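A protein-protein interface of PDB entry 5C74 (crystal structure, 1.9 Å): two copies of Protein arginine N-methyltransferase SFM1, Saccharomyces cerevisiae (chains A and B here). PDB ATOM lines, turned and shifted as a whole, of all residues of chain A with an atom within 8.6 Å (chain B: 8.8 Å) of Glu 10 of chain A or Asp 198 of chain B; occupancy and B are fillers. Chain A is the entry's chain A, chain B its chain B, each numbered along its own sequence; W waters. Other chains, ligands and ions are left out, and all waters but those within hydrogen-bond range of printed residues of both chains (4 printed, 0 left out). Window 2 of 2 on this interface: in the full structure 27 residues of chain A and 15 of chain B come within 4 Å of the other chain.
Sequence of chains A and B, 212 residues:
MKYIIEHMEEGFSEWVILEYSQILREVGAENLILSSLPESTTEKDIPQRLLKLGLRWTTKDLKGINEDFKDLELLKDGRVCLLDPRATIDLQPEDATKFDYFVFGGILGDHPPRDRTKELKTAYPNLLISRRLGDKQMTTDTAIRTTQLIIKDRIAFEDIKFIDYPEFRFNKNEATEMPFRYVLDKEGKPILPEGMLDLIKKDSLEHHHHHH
The side-chain carboxylate (OE2) of Glu 9 of chain A lies within salt-bridge range of the side-chain amino group (NZ) of Lys 201 of chain B (3.9 Å). The backbone carbonyl oxygen (O) of Phe 12 of chain A lies within hydrogen-bond range of the side-chain amino group (NZ) of Lys 202 of chain B. The backbone NH of Glu 14 of chain A lies within hydrogen-bond range of the backbone carbonyl oxygen of Lys 202 of chain B, 3.0 Å away.
Among the printed residues, merely in contact across the chains: Ser 13 of chain A with Lys 202 of chain B (3.4 Å), Glu 10 of chain A with Asp 198 of chain B (3.7 Å) and Ser 13 of chain A with Lys 201 of chain B (3.9 Å).
Of the printed residues of chain B, Glu 9 of chain A touches Lys 201. Glu 10 of chain A touches just one residue of chain B: Asp 198 (3.7 Å). No residue of chain B comes within 4 Å of Gly 11 of chain A. Printed residues of chain B within 4 Å of Phe 12 of chain A: Lys 202 (2.6 Å). Leu 18 of chain B touches none of the printed residues of chain A. Asp 198 of chain B touches just one residue of chain A: Glu 10.
Printed residues of chain B that touch a printed residue of chain A: Asp 198, Lys 201 and Lys 202. Of the 18 printed residues of chain A, 5 touch a printed residue of chain B. Printed residues of chain A that touch a printed residue of chain B: Glu 9, Glu 10, Phe 12, Ser 13 and Glu 14. Among the printed residues, Asp or Glu carboxylates within 4 Å of a Lys or Arg side-chain nitrogen of the other chain: Glu 9 of chain A with Lys 201 of chain B.
Position printed for both chains: 14. Of the 6 pairs that touch across the chains among the printed residues, none has its exchanged pair printed and touching as well.
Water W2 bridges O of Glu 10 of chain A and OD1 of Asp 198 of chain B. Water W3 bridges the side-chain carboxylate (OE1) of Glu 14 of chain A (2.5 Å) and the side-chain amino group (NZ) of Lys 202 of chain B (3.4 Å). Water W1 bridges N of Phe 12 of chain A and NZ of Lys 202 of chain B. Water W4 lies within hydrogen-bond range of O of Lys 202 of chain B (3.1 Å), O of Ser 204 of chain B (3.2 Å) and N of Glu 14 of chain A (3.3 Å).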
ATOM      1  N   HIS A   7      12.195  -3.270  -0.857  1.00  0.00           N
ATOM      2  CA  HIS A   7      12.502  -4.661  -1.155  1.00  0.00           C
ATOM      3  C   HIS A   7      13.853  -4.928  -0.537  1.00  0.00           C
ATOM      4  O   HIS A   7      14.855  -4.872  -1.220  1.00  0.00           O
ATOM      5  CB  HIS A   7      12.510  -4.925  -2.668  1.00  0.00           C
ATOM      6  CG  HIS A   7      12.687  -6.374  -3.029  1.00  0.00           C
ATOM      7  ND1 HIS A   7      11.624  -7.201  -3.329  1.00  0.00           N
ATOM      8  CD2 HIS A   7      13.803  -7.143  -3.129  1.00  0.00           C
ATOM      9  CE1 HIS A   7      12.076  -8.418  -3.598  1.00  0.00           C
ATOM     10  NE2 HIS A   7      13.395  -8.407  -3.486  1.00  0.00           N
ATOM     11  N   MET A   8      13.866  -5.182   0.767  1.00  0.00           N
ATOM     12  CA  MET A   8      15.107  -5.210   1.533  1.00  0.00           C
ATOM     13  C   MET A   8      15.571  -6.638   1.773  1.00  0.00           C
ATOM     14  O   MET A   8      15.826  -7.047   2.908  1.00  0.00           O
ATOM     15  CB  MET A   8      14.929  -4.487   2.870  1.00  0.00           C
ATOM     16  CG  MET A   8      14.540  -2.991   2.742  1.00  0.00           C
ATOM     17  SD  MET A   8      14.155  -2.167   4.323  1.00  0.00           S
ATOM     18  CE  MET A   8      15.785  -2.043   5.053  1.00  0.00           C
ATOM     19  N   GLU A   9      15.655  -7.401   0.700  1.00  0.00           N
ATOM     20  CA  GLU A   9      16.075  -8.785   0.805  1.00  0.00           C
ATOM     21  C   GLU A   9      16.749  -9.137  -0.491  1.00  0.00           C
ATOM     22  O   GLU A   9      16.483  -8.537  -1.532  1.00  0.00           O
ATOM     23  CB  GLU A   9      14.886  -9.719   1.075  1.00  0.00           C
ATOM     24  CG  GLU A   9      13.926  -9.838  -0.108  1.00  0.00           C
ATOM     25  CD  GLU A   9      12.688 -10.672   0.196  1.00  0.00           C
ATOM     26  OE1 GLU A   9      11.635 -10.412  -0.428  1.00  0.00           O
ATOM     27  OE2 GLU A   9      12.767 -11.587   1.045  1.00  0.00           O
ATOM     28  N   GLU A  10      17.648 -10.103  -0.426  1.00  0.00           N
ATOM     29  CA  GLU A  10      18.309 -10.586  -1.615  1.00  0.00           C
ATOM     30  C   GLU A  10      17.335 -11.475  -2.387  1.00  0.00           C
ATOM     31  O   GLU A  10      16.673 -12.321  -1.792  1.00  0.00           O
ATOM     32  CB  GLU A  10      19.563 -11.371  -1.232  1.00  0.00           C
ATOM     33  CG  GLU A  10      20.367 -11.840  -2.402  1.00  0.00           C
ATOM     34  CD  GLU A  10      20.879 -10.688  -3.226  1.00  0.00           C
ATOM     35  OE1 GLU A  10      20.904 -10.820  -4.467  1.00  0.00           O
ATOM     36  OE2 GLU A  10      21.258  -9.657  -2.626  1.00  0.00           O
ATOM     37  N   GLY A  11      17.241 -11.277  -3.697  1.00  0.00           N
ATOM     38  CA  GLY A  11      16.487 -12.187  -4.536  1.00  0.00           C
ATOM     39  C   GLY A  11      15.016 -11.860  -4.705  1.00  0.00           C
ATOM     40  O   GLY A  11      14.427 -11.126  -3.913  1.00  0.00           O
ATOM     41  N   PHE A  12      14.434 -12.418  -5.758  1.00  0.00           N
ATOM     42  CA  PHE A  12      13.012 -12.301  -6.043  1.00  0.00           C
ATOM     43  C   PHE A  12      12.428 -13.693  -6.147  1.00  0.00           C
ATOM     44  O   PHE A  12      12.719 -14.405  -7.096  1.00  0.00           O
ATOM     45  CB  PHE A  12      12.767 -11.553  -7.355  1.00  0.00           C
ATOM     46  CG  PHE A  12      13.201 -10.112  -7.331  1.00  0.00           C
ATOM     47  CD1 PHE A  12      14.547  -9.776  -7.415  1.00  0.00           C
ATOM     48  CD2 PHE A  12      12.257  -9.098  -7.258  1.00  0.00           C
ATOM     49  CE1 PHE A  12      14.951  -8.453  -7.401  1.00  0.00           C
ATOM     50  CE2 PHE A  12      12.653  -7.761  -7.243  1.00  0.00           C
ATOM     51  CZ  PHE A  12      13.995  -7.441  -7.308  1.00  0.00           C
ATOM     52  N   SER A  13      11.608 -14.071  -5.179  1.00  0.00           N
ATOM     53  CA  SER A  13      10.933 -15.362  -5.250  1.00  0.00           C
ATOM     54  C   SER A  13       9.917 -15.362  -6.388  1.00  0.00           C
ATOM     55  O   SER A  13       9.472 -14.304  -6.832  1.00  0.00           O
ATOM     56  CB  SER A  13      10.246 -15.669  -3.938  1.00  0.00           C
ATOM     57  OG  SER A  13       9.152 -14.789  -3.775  1.00  0.00           O
ATOM     58  N   GLU A  14       9.547 -16.545  -6.862  1.00  0.00           N
ATOM     59  CA  GLU A  14       8.637 -16.622  -7.989  1.00  0.00           C
ATOM     60  C   GLU A  14       7.298 -15.968  -7.651  1.00  0.00           C
ATOM     61  O   GLU A  14       6.743 -15.241  -8.478  1.00  0.00           O
ATOM     62  CB  GLU A  14       8.446 -18.080  -8.426  1.00  0.00           C
ATOM     63  CG  GLU A  14       7.538 -18.263  -9.631  1.00  0.00           C
ATOM     64  CD  GLU A  14       8.069 -17.613 -10.910  1.00  0.00           C
ATOM     65  OE1 GLU A  14       9.282 -17.293 -10.991  1.00  0.00           O
ATOM     66  OE2 GLU A  14       7.257 -17.426 -11.842  1.00  0.00           O
ATOM     67  N   SER A  36      15.440   0.647  -1.423  1.00  0.00           N
ATOM     68  CA  SER A  36      16.305  -0.005  -0.441  1.00  0.00           C
ATOM     69  C   SER A  36      16.679  -1.440  -0.820  1.00  0.00           C
ATOM     70  O   SER A  36      16.869  -2.274   0.066  1.00  0.00           O
ATOM     71  CB  SER A  36      15.660   0.017   0.955  1.00  0.00           C
ATOM     72  OG  SER A  36      15.532   1.364   1.412  1.00  0.00           O
ATOM     73  N   LEU A  37      16.836  -1.708  -2.116  1.00  0.00           N
ATOM     74  CA  LEU A  37      17.430  -2.983  -2.545  1.00  0.00           C
ATOM     75  C   LEU A  37      18.824  -3.131  -1.949  1.00  0.00           C
ATOM     76  O   LEU A  37      19.503  -2.125  -1.698  1.00  0.00           O
ATOM     77  CB  LEU A  37      17.501  -3.078  -4.073  1.00  0.00           C
ATOM     78  CG  LEU A  37      16.205  -3.711  -4.612  1.00  0.00           C
ATOM     79  CD1 LEU A  37      15.059  -2.689  -4.624  1.00  0.00           C
ATOM     80  CD2 LEU A  37      16.389  -4.322  -5.973  1.00  0.00           C
ATOM     81  N   PRO A  38      19.263  -4.383  -1.728  1.00  0.00           N
ATOM     82  CA  PRO A  38      20.616  -4.630  -1.220  1.00  0.00           C
ATOM     83  C   PRO A  38      21.669  -3.906  -2.048  1.00  0.00           C
ATOM     84  O   PRO A  38      21.542  -3.752  -3.272  1.00  0.00           O
ATOM     85  CB  PRO A  38      20.763  -6.153  -1.330  1.00  0.00           C
ATOM     86  CG  PRO A  38      19.342  -6.662  -1.210  1.00  0.00           C
ATOM     87  CD  PRO A  38      18.526  -5.637  -1.971  1.00  0.00           C
ATOM     88  N   GLU A  39      22.707  -3.439  -1.365  1.00  0.00           N
ATOM     89  CA  GLU A  39      23.687  -2.578  -2.004  1.00  0.00           C
ATOM     90  C   GLU A  39      24.378  -3.245  -3.200  1.00  0.00           C
ATOM     91  O   GLU A  39      24.856  -2.565  -4.102  1.00  0.00           O
ATOM     92  CB  GLU A  39      24.726  -2.126  -0.971  1.00  0.00           C
ATOM     93  CG  GLU A  39      25.378  -0.792  -1.301  1.00  0.00           C
ATOM     94  CD  GLU A  39      24.460   0.418  -1.059  1.00  0.00           C
ATOM     95  OE1 GLU A  39      23.279   0.256  -0.688  1.00  0.00           O
ATOM     96  OE2 GLU A  39      24.933   1.557  -1.239  1.00  0.00           O
ATOM     97  N   SER A  40      24.405  -4.574  -3.217  1.00  0.00           N
ATOM     98  CA  SER A  40      25.108  -5.320  -4.265  1.00  0.00           C
ATOM     99  C   SER A  40      24.270  -5.501  -5.525  1.00  0.00           C
ATOM    100  O   SER A  40      24.723  -6.096  -6.499  1.00  0.00           O
ATOM    101  CB  SER A  40      25.528  -6.701  -3.741  1.00  0.00           C
ATOM    102  OG  SER A  40      26.399  -6.575  -2.633  1.00  0.00           O
ATOM    103  N   THR A  41      23.047  -4.991  -5.515  1.00  0.00           N
ATOM    104  CA  THR A  41      22.135  -5.217  -6.634  1.00  0.00           C
ATOM    105  C   THR A  41      22.564  -4.499  -7.905  1.00  0.00           C
ATOM    106  O   THR A  41      22.909  -3.322  -7.869  1.00  0.00           O
ATOM    107  CB  THR A  41      20.706  -4.764  -6.266  1.00  0.00           C
ATOM    108  OG1 THR A  41      20.348  -5.352  -5.016  1.00  0.00           O
ATOM    109  CG2 THR A  41      19.710  -5.171  -7.338  1.00  0.00           C
ATOM    110  N   THR A  42      22.560  -5.210  -9.029  1.00  0.00           N
ATOM    111  CA  THR A  42      22.734  -4.568 -10.324  1.00  0.00           C
ATOM    112  C   THR A  42      21.584  -5.005 -11.211  1.00  0.00           C
ATOM    113  O   THR A  42      20.768  -5.839 -10.813  1.00  0.00           O
ATOM    114  CB  THR A  42      24.086  -4.909 -11.004  1.00  0.00           C
ATOM    115  OG1 THR A  42      24.076  -6.259 -11.480  1.00  0.00           O
ATOM    116  CG2 THR A  42      25.238  -4.726 -10.033  1.00  0.00           C
ATOM    117  N   LYS A  44      21.521  -6.963 -13.545  1.00  0.00           N
ATOM    118  CA  LYS A  44      21.566  -8.406 -13.792  1.00  0.00           C
ATOM    119  C   LYS A  44      20.787  -9.208 -12.748  1.00  0.00           C
ATOM    120  O   LYS A  44      20.403 -10.358 -12.985  1.00  0.00           O
ATOM    121  CB  LYS A  44      23.020  -8.892 -13.835  1.00  0.00           C
ATOM    122  CG  LYS A  44      23.840  -8.249 -14.927  1.00  0.00           C
ATOM    123  CD  LYS A  44      25.323  -8.561 -14.770  1.00  0.00           C
ATOM    124  CE  LYS A  44      26.125  -7.989 -15.930  1.00  0.00           C
ATOM    125  NZ  LYS A  44      27.588  -8.225 -15.768  1.00  0.00           N
ATOM    126  N   ASP A  45      20.556  -8.603 -11.590  1.00  0.00           N
ATOM    127  CA  ASP A  45      19.832  -9.288 -10.521  1.00  0.00           C
ATOM    128  C   ASP A  45      18.315  -9.169 -10.636  1.00  0.00           C
ATOM    129  O   ASP A  45      17.578  -9.830  -9.892  1.00  0.00           O
ATOM    130  CB  ASP A  45      20.266  -8.752  -9.160  1.00  0.00           C
ATOM    131  CG  ASP A  45      21.722  -9.059  -8.849  1.00  0.00           C
ATOM    132  OD1 ASP A  45      22.061 -10.253  -8.774  1.00  0.00           O
ATOM    133  OD2 ASP A  45      22.517  -8.114  -8.648  1.00  0.00           O
ATOM    134  N   ILE A  46      17.847  -8.317 -11.538  1.00  0.00           N
ATOM    135  CA  ILE A  46      16.407  -8.091 -11.669  1.00  0.00           C
ATOM    136  C   ILE A  46      15.806  -9.084 -12.649  1.00  0.00           C
ATOM    137  O   ILE A  46      16.304  -9.228 -13.767  1.00  0.00           O
ATOM    138  CB  ILE A  46      16.103  -6.656 -12.140  1.00  0.00           C
ATOM    139  CG1 ILE A  46      16.936  -5.650 -11.337  1.00  0.00           C
ATOM    140  CG2 ILE A  46      14.604  -6.352 -12.030  1.00  0.00           C
ATOM    141  CD1 ILE A  46      16.570  -5.586  -9.852  1.00  0.00           C
ATOM    142  N   GLU B  14      20.816 -23.624 -11.996  1.00  0.00           N
ATOM    143  CA  GLU B  14      21.404 -22.717 -11.014  1.00  0.00           C
ATOM    144  C   GLU B  14      21.792 -23.487  -9.759  1.00  0.00           C
ATOM    145  O   GLU B  14      22.840 -23.225  -9.163  1.00  0.00           O
ATOM    146  CB  GLU B  14      20.450 -21.583 -10.665  1.00  0.00           C
ATOM    147  CG  GLU B  14      21.035 -20.571  -9.681  1.00  0.00           C
ATOM    148  CD  GLU B  14      22.160 -19.726 -10.283  1.00  0.00           C
ATOM    149  OE1 GLU B  14      22.868 -19.051  -9.510  1.00  0.00           O
ATOM    150  OE2 GLU B  14      22.332 -19.728 -11.521  1.00  0.00           O
ATOM    151  N   LEU B  18      25.628 -23.647  -8.243  1.00  0.00           N
ATOM    152  CA  LEU B  18      25.949 -23.360  -6.846  1.00  0.00           C
ATOM    153  C   LEU B  18      26.621 -24.541  -6.163  1.00  0.00           C
ATOM    154  O   LEU B  18      27.534 -24.354  -5.357  1.00  0.00           O
ATOM    155  CB  LEU B  18      24.691 -22.983  -6.063  1.00  0.00           C
ATOM    156  CG  LEU B  18      23.937 -21.752  -6.553  1.00  0.00           C
ATOM    157  CD1 LEU B  18      22.748 -21.489  -5.627  1.00  0.00           C
ATOM    158  CD2 LEU B  18      24.861 -20.542  -6.638  1.00  0.00           C
ATOM    159  N   PHE B 168      13.798 -25.663   6.595  1.00  0.00           N
ATOM    160  CA  PHE B 168      14.279 -24.289   6.606  1.00  0.00           C
ATOM    161  C   PHE B 168      13.102 -23.349   6.763  1.00  0.00           C
ATOM    162  O   PHE B 168      12.151 -23.403   5.982  1.00  0.00           O
ATOM    163  CB  PHE B 168      15.068 -23.974   5.334  1.00  0.00           C
ATOM    164  CG  PHE B 168      16.277 -24.849   5.159  1.00  0.00           C
ATOM    165  CD1 PHE B 168      17.492 -24.483   5.708  1.00  0.00           C
ATOM    166  CD2 PHE B 168      16.187 -26.052   4.477  1.00  0.00           C
ATOM    167  CE1 PHE B 168      18.608 -25.291   5.562  1.00  0.00           C
ATOM    168  CE2 PHE B 168      17.293 -26.869   4.331  1.00  0.00           C
ATOM    169  CZ  PHE B 168      18.508 -26.487   4.878  1.00  0.00           C
ATOM    170  N   PHE B 170      11.813 -19.407   6.870  1.00  0.00           N
ATOM    171  CA  PHE B 170      12.177 -18.098   6.345  1.00  0.00           C
ATOM    172  C   PHE B 170      11.292 -17.008   6.929  1.00  0.00           C
ATOM    173  O   PHE B 170      10.459 -17.256   7.803  1.00  0.00           O
ATOM    174  CB  PHE B 170      12.069 -18.069   4.816  1.00  0.00           C
ATOM    175  CG  PHE B 170      12.742 -19.224   4.136  1.00  0.00           C
ATOM    176  CD1 PHE B 170      14.122 -19.338   4.140  1.00  0.00           C
ATOM    177  CD2 PHE B 170      12.000 -20.183   3.471  1.00  0.00           C
ATOM    178  CE1 PHE B 170      14.749 -20.398   3.510  1.00  0.00           C
ATOM    179  CE2 PHE B 170      12.618 -21.243   2.838  1.00  0.00           C
ATOM    180  CZ  PHE B 170      13.996 -21.352   2.857  1.00  0.00           C
ATOM    181  N   LEU B 192      25.208 -25.641   3.533  1.00  0.00           N
ATOM    182  CA  LEU B 192      24.748 -25.518   2.160  1.00  0.00           C
ATOM    183  C   LEU B 192      25.776 -24.801   1.301  1.00  0.00           C
ATOM    184  O   LEU B 192      26.562 -24.002   1.809  1.00  0.00           O
ATOM    185  CB  LEU B 192      23.435 -24.737   2.103  1.00  0.00           C
ATOM    186  CG  LEU B 192      22.269 -25.191   2.960  1.00  0.00           C
ATOM    187  CD1 LEU B 192      21.111 -24.200   2.774  1.00  0.00           C
ATOM    188  CD2 LEU B 192      21.857 -26.579   2.554  1.00  0.00           C
ATOM    189  N   PRO B 193      25.754 -25.053  -0.016  1.00  0.00           N
ATOM    190  CA  PRO B 193      26.504 -24.183  -0.927  1.00  0.00           C
ATOM    191  C   PRO B 193      26.135 -22.722  -0.719  1.00  0.00           C
ATOM    192  O   PRO B 193      24.993 -22.421  -0.358  1.00  0.00           O
ATOM    193  CB  PRO B 193      26.063 -24.660  -2.313  1.00  0.00           C
ATOM    194  CG  PRO B 193      25.696 -26.091  -2.108  1.00  0.00           C
ATOM    195  CD  PRO B 193      25.085 -26.154  -0.725  1.00  0.00           C
ATOM    196  N   GLU B 194      27.094 -21.825  -0.926  1.00  0.00           N
ATOM    197  CA  GLU B 194      26.803 -20.403  -0.925  1.00  0.00           C
ATOM    198  C   GLU B 194      25.707 -20.109  -1.942  1.00  0.00           C
ATOM    199  O   GLU B 194      25.741 -20.604  -3.068  1.00  0.00           O
ATOM    200  CB  GLU B 194      28.061 -19.577  -1.238  1.00  0.00           C
ATOM    201  CG  GLU B 194      29.123 -19.637  -0.153  1.00  0.00           C
ATOM    202  CD  GLU B 194      30.333 -18.759  -0.449  1.00  0.00           C
ATOM    203  OE1 GLU B 194      30.339 -18.064  -1.489  1.00  0.00           O
ATOM    204  OE2 GLU B 194      31.280 -18.776   0.364  1.00  0.00           O
ATOM    205  N   GLY B 195      24.727 -19.309  -1.534  1.00  0.00           N
ATOM    206  CA  GLY B 195      23.616 -18.979  -2.403  1.00  0.00           C
ATOM    207  C   GLY B 195      22.468 -19.983  -2.438  1.00  0.00           C
ATOM    208  O   GLY B 195      21.409 -19.679  -3.000  1.00  0.00           O
ATOM    209  N   MET B 196      22.653 -21.168  -1.855  1.00  0.00           N
ATOM    210  CA  MET B 196      21.629 -22.221  -1.949  1.00  0.00           C
ATOM    211  C   MET B 196      20.380 -21.869  -1.154  1.00  0.00           C
ATOM    212  O   MET B 196      19.256 -22.130  -1.592  1.00  0.00           O
ATOM    213  CB  MET B 196      22.188 -23.575  -1.471  1.00  0.00           C
ATOM    214  CG  MET B 196      21.168 -24.741  -1.509  1.00  0.00           C
ATOM    215  SD  MET B 196      20.526 -25.071  -3.169  1.00  0.00           S
ATOM    216  CE  MET B 196      22.021 -25.621  -3.981  1.00  0.00           C
ATOM    217  N   LEU B 197      20.576 -21.281   0.021  1.00  0.00           N
ATOM    218  CA  LEU B 197      19.451 -20.875   0.851  1.00  0.00           C
ATOM    219  C   LEU B 197      18.553 -19.881   0.104  1.00  0.00           C
ATOM    220  O   LEU B 197      17.336 -20.004   0.128  1.00  0.00           O
ATOM    221  CB  LEU B 197      19.955 -20.279   2.165  1.00  0.00           C
ATOM    222  CG  LEU B 197      18.971 -20.178   3.329  1.00  0.00           C
ATOM    223  CD1 LEU B 197      18.175 -21.469   3.468  1.00  0.00           C
ATOM    224  CD2 LEU B 197      19.724 -19.889   4.617  1.00  0.00           C
ATOM    225  N   ASP B 198      19.152 -18.908  -0.580  1.00  0.00           N
ATOM    226  CA  ASP B 198      18.373 -17.950  -1.374  1.00  0.00           C
ATOM    227  C   ASP B 198      17.618 -18.650  -2.512  1.00  0.00           C
ATOM    228  O   ASP B 198      16.502 -18.264  -2.856  1.00  0.00           O
ATOM    229  CB  ASP B 198      19.272 -16.854  -1.964  1.00  0.00           C
ATOM    230  CG  ASP B 198      19.832 -15.910  -0.911  1.00  0.00           C
ATOM    231  OD1 ASP B 198      19.250 -15.820   0.191  1.00  0.00           O
ATOM    232  OD2 ASP B 198      20.859 -15.252  -1.195  1.00  0.00           O
ATOM    233  N   LEU B 199      18.235 -19.669  -3.104  1.00  0.00           N
ATOM    234  CA  LEU B 199      17.599 -20.406  -4.192  1.00  0.00           C
ATOM    235  C   LEU B 199      16.427 -21.232  -3.668  1.00  0.00           C
ATOM    236  O   LEU B 199      15.397 -21.347  -4.331  1.00  0.00           O
ATOM    237  CB  LEU B 199      18.606 -21.314  -4.905  1.00  0.00           C
ATOM    238  CG  LEU B 199      18.109 -22.162  -6.080  1.00  0.00           C
ATOM    239  CD1 LEU B 199      17.484 -21.297  -7.174  1.00  0.00           C
ATOM    240  CD2 LEU B 199      19.264 -23.002  -6.650  1.00  0.00           C
ATOM    241  N   ILE B 200      16.583 -21.802  -2.476  1.00  0.00           N
ATOM    242  CA  ILE B 200      15.482 -22.531  -1.848  1.00  0.00           C
ATOM    243  C   ILE B 200      14.334 -21.552  -1.571  1.00  0.00           C
ATOM    244  O   ILE B 200      13.167 -21.826  -1.876  1.00  0.00           O
ATOM    245  CB  ILE B 200      15.937 -23.233  -0.553  1.00  0.00           C
ATOM    246  CG1 ILE B 200      16.989 -24.304  -0.894  1.00  0.00           C
ATOM    247  CG2 ILE B 200      14.759 -23.852   0.175  1.00  0.00           C
ATOM    248  CD1 ILE B 200      17.598 -25.016   0.305  1.00  0.00           C
ATOM    249  N   LYS B 201      14.681 -20.397  -1.024  1.00  0.00           N
ATOM    250  CA  LYS B 201      13.695 -19.354  -0.731  1.00  0.00           C
ATOM    251  C   LYS B 201      12.956 -18.924  -2.002  1.00  0.00           C
ATOM    252  O   LYS B 201      11.758 -18.652  -1.979  1.00  0.00           O
ATOM    253  CB  LYS B 201      14.390 -18.156  -0.073  1.00  0.00           C
ATOM    254  CG  LYS B 201      13.454 -17.068   0.425  1.00  0.00           C
ATOM    255  CD  LYS B 201      14.225 -15.984   1.168  1.00  0.00           C
ATOM    256  CE  LYS B 201      13.330 -14.793   1.497  1.00  0.00           C
ATOM    257  NZ  LYS B 201      12.167 -15.199   2.339  1.00  0.00           N
ATOM    258  N   LYS B 202      13.674 -18.902  -3.118  1.00  0.00           N
ATOM    259  CA  LYS B 202      13.120 -18.408  -4.374  1.00  0.00           C
ATOM    260  C   LYS B 202      11.955 -19.270  -4.848  1.00  0.00           C
ATOM    261  O   LYS B 202      11.012 -18.765  -5.465  1.00  0.00           O
ATOM    262  CB  LYS B 202      14.215 -18.345  -5.442  1.00  0.00           C
ATOM    263  CG  LYS B 202      13.800 -17.751  -6.787  1.00  0.00           C
ATOM    264  CD  LYS B 202      15.037 -17.563  -7.682  1.00  0.00           C
ATOM    265  CE  LYS B 202      14.688 -16.965  -9.045  1.00  0.00           C
ATOM    266  NZ  LYS B 202      14.106 -15.587  -8.957  1.00  0.00           N
ATOM    267  N   ASP B 203      12.008 -20.567  -4.547  1.00  0.00           N
ATOM    268  CA  ASP B 203      10.950 -21.482  -4.967  1.00  0.00           C
ATOM    269  C   ASP B 203       9.946 -21.802  -3.858  1.00  0.00           C
ATOM    270  O   ASP B 203       9.045 -22.615  -4.060  1.00  0.00           O
ATOM    271  CB  ASP B 203      11.549 -22.793  -5.492  1.00  0.00           C
ATOM    272  CG  ASP B 203      11.899 -22.728  -6.965  1.00  0.00           C
ATOM    273  OD1 ASP B 203      11.251 -21.937  -7.693  1.00  0.00           O
ATOM    274  OD2 ASP B 203      12.812 -23.475  -7.389  1.00  0.00           O
ATOM    275  N   SER B 204      10.104 -21.177  -2.695  1.00  0.00           N
ATOM    276  CA  SER B 204       9.155 -21.363  -1.604  1.00  0.00           C
ATOM    277  C   SER B 204       7.909 -20.510  -1.808  1.00  0.00           C
ATOM    278  O   SER B 204       8.019 -19.315  -2.012  1.00  0.00           O
ATOM    279  CB  SER B 204       9.796 -21.012  -0.264  1.00  0.00           C
ATOM    280  OG  SER B 204      10.939 -21.816  -0.030  1.00  0.00           O
HETATM  281  O   HOH W   1      16.302 -13.823  -7.411  1.00  0.00           O
HETATM  282  O   HOH W   2      16.835 -13.494   0.458  1.00  0.00           O
HETATM  283  O   HOH W   3      11.648 -17.560 -10.100  1.00  0.00           O
HETATM  284  O   HOH W   4       7.934 -18.874  -5.161  1.00  0.00           O
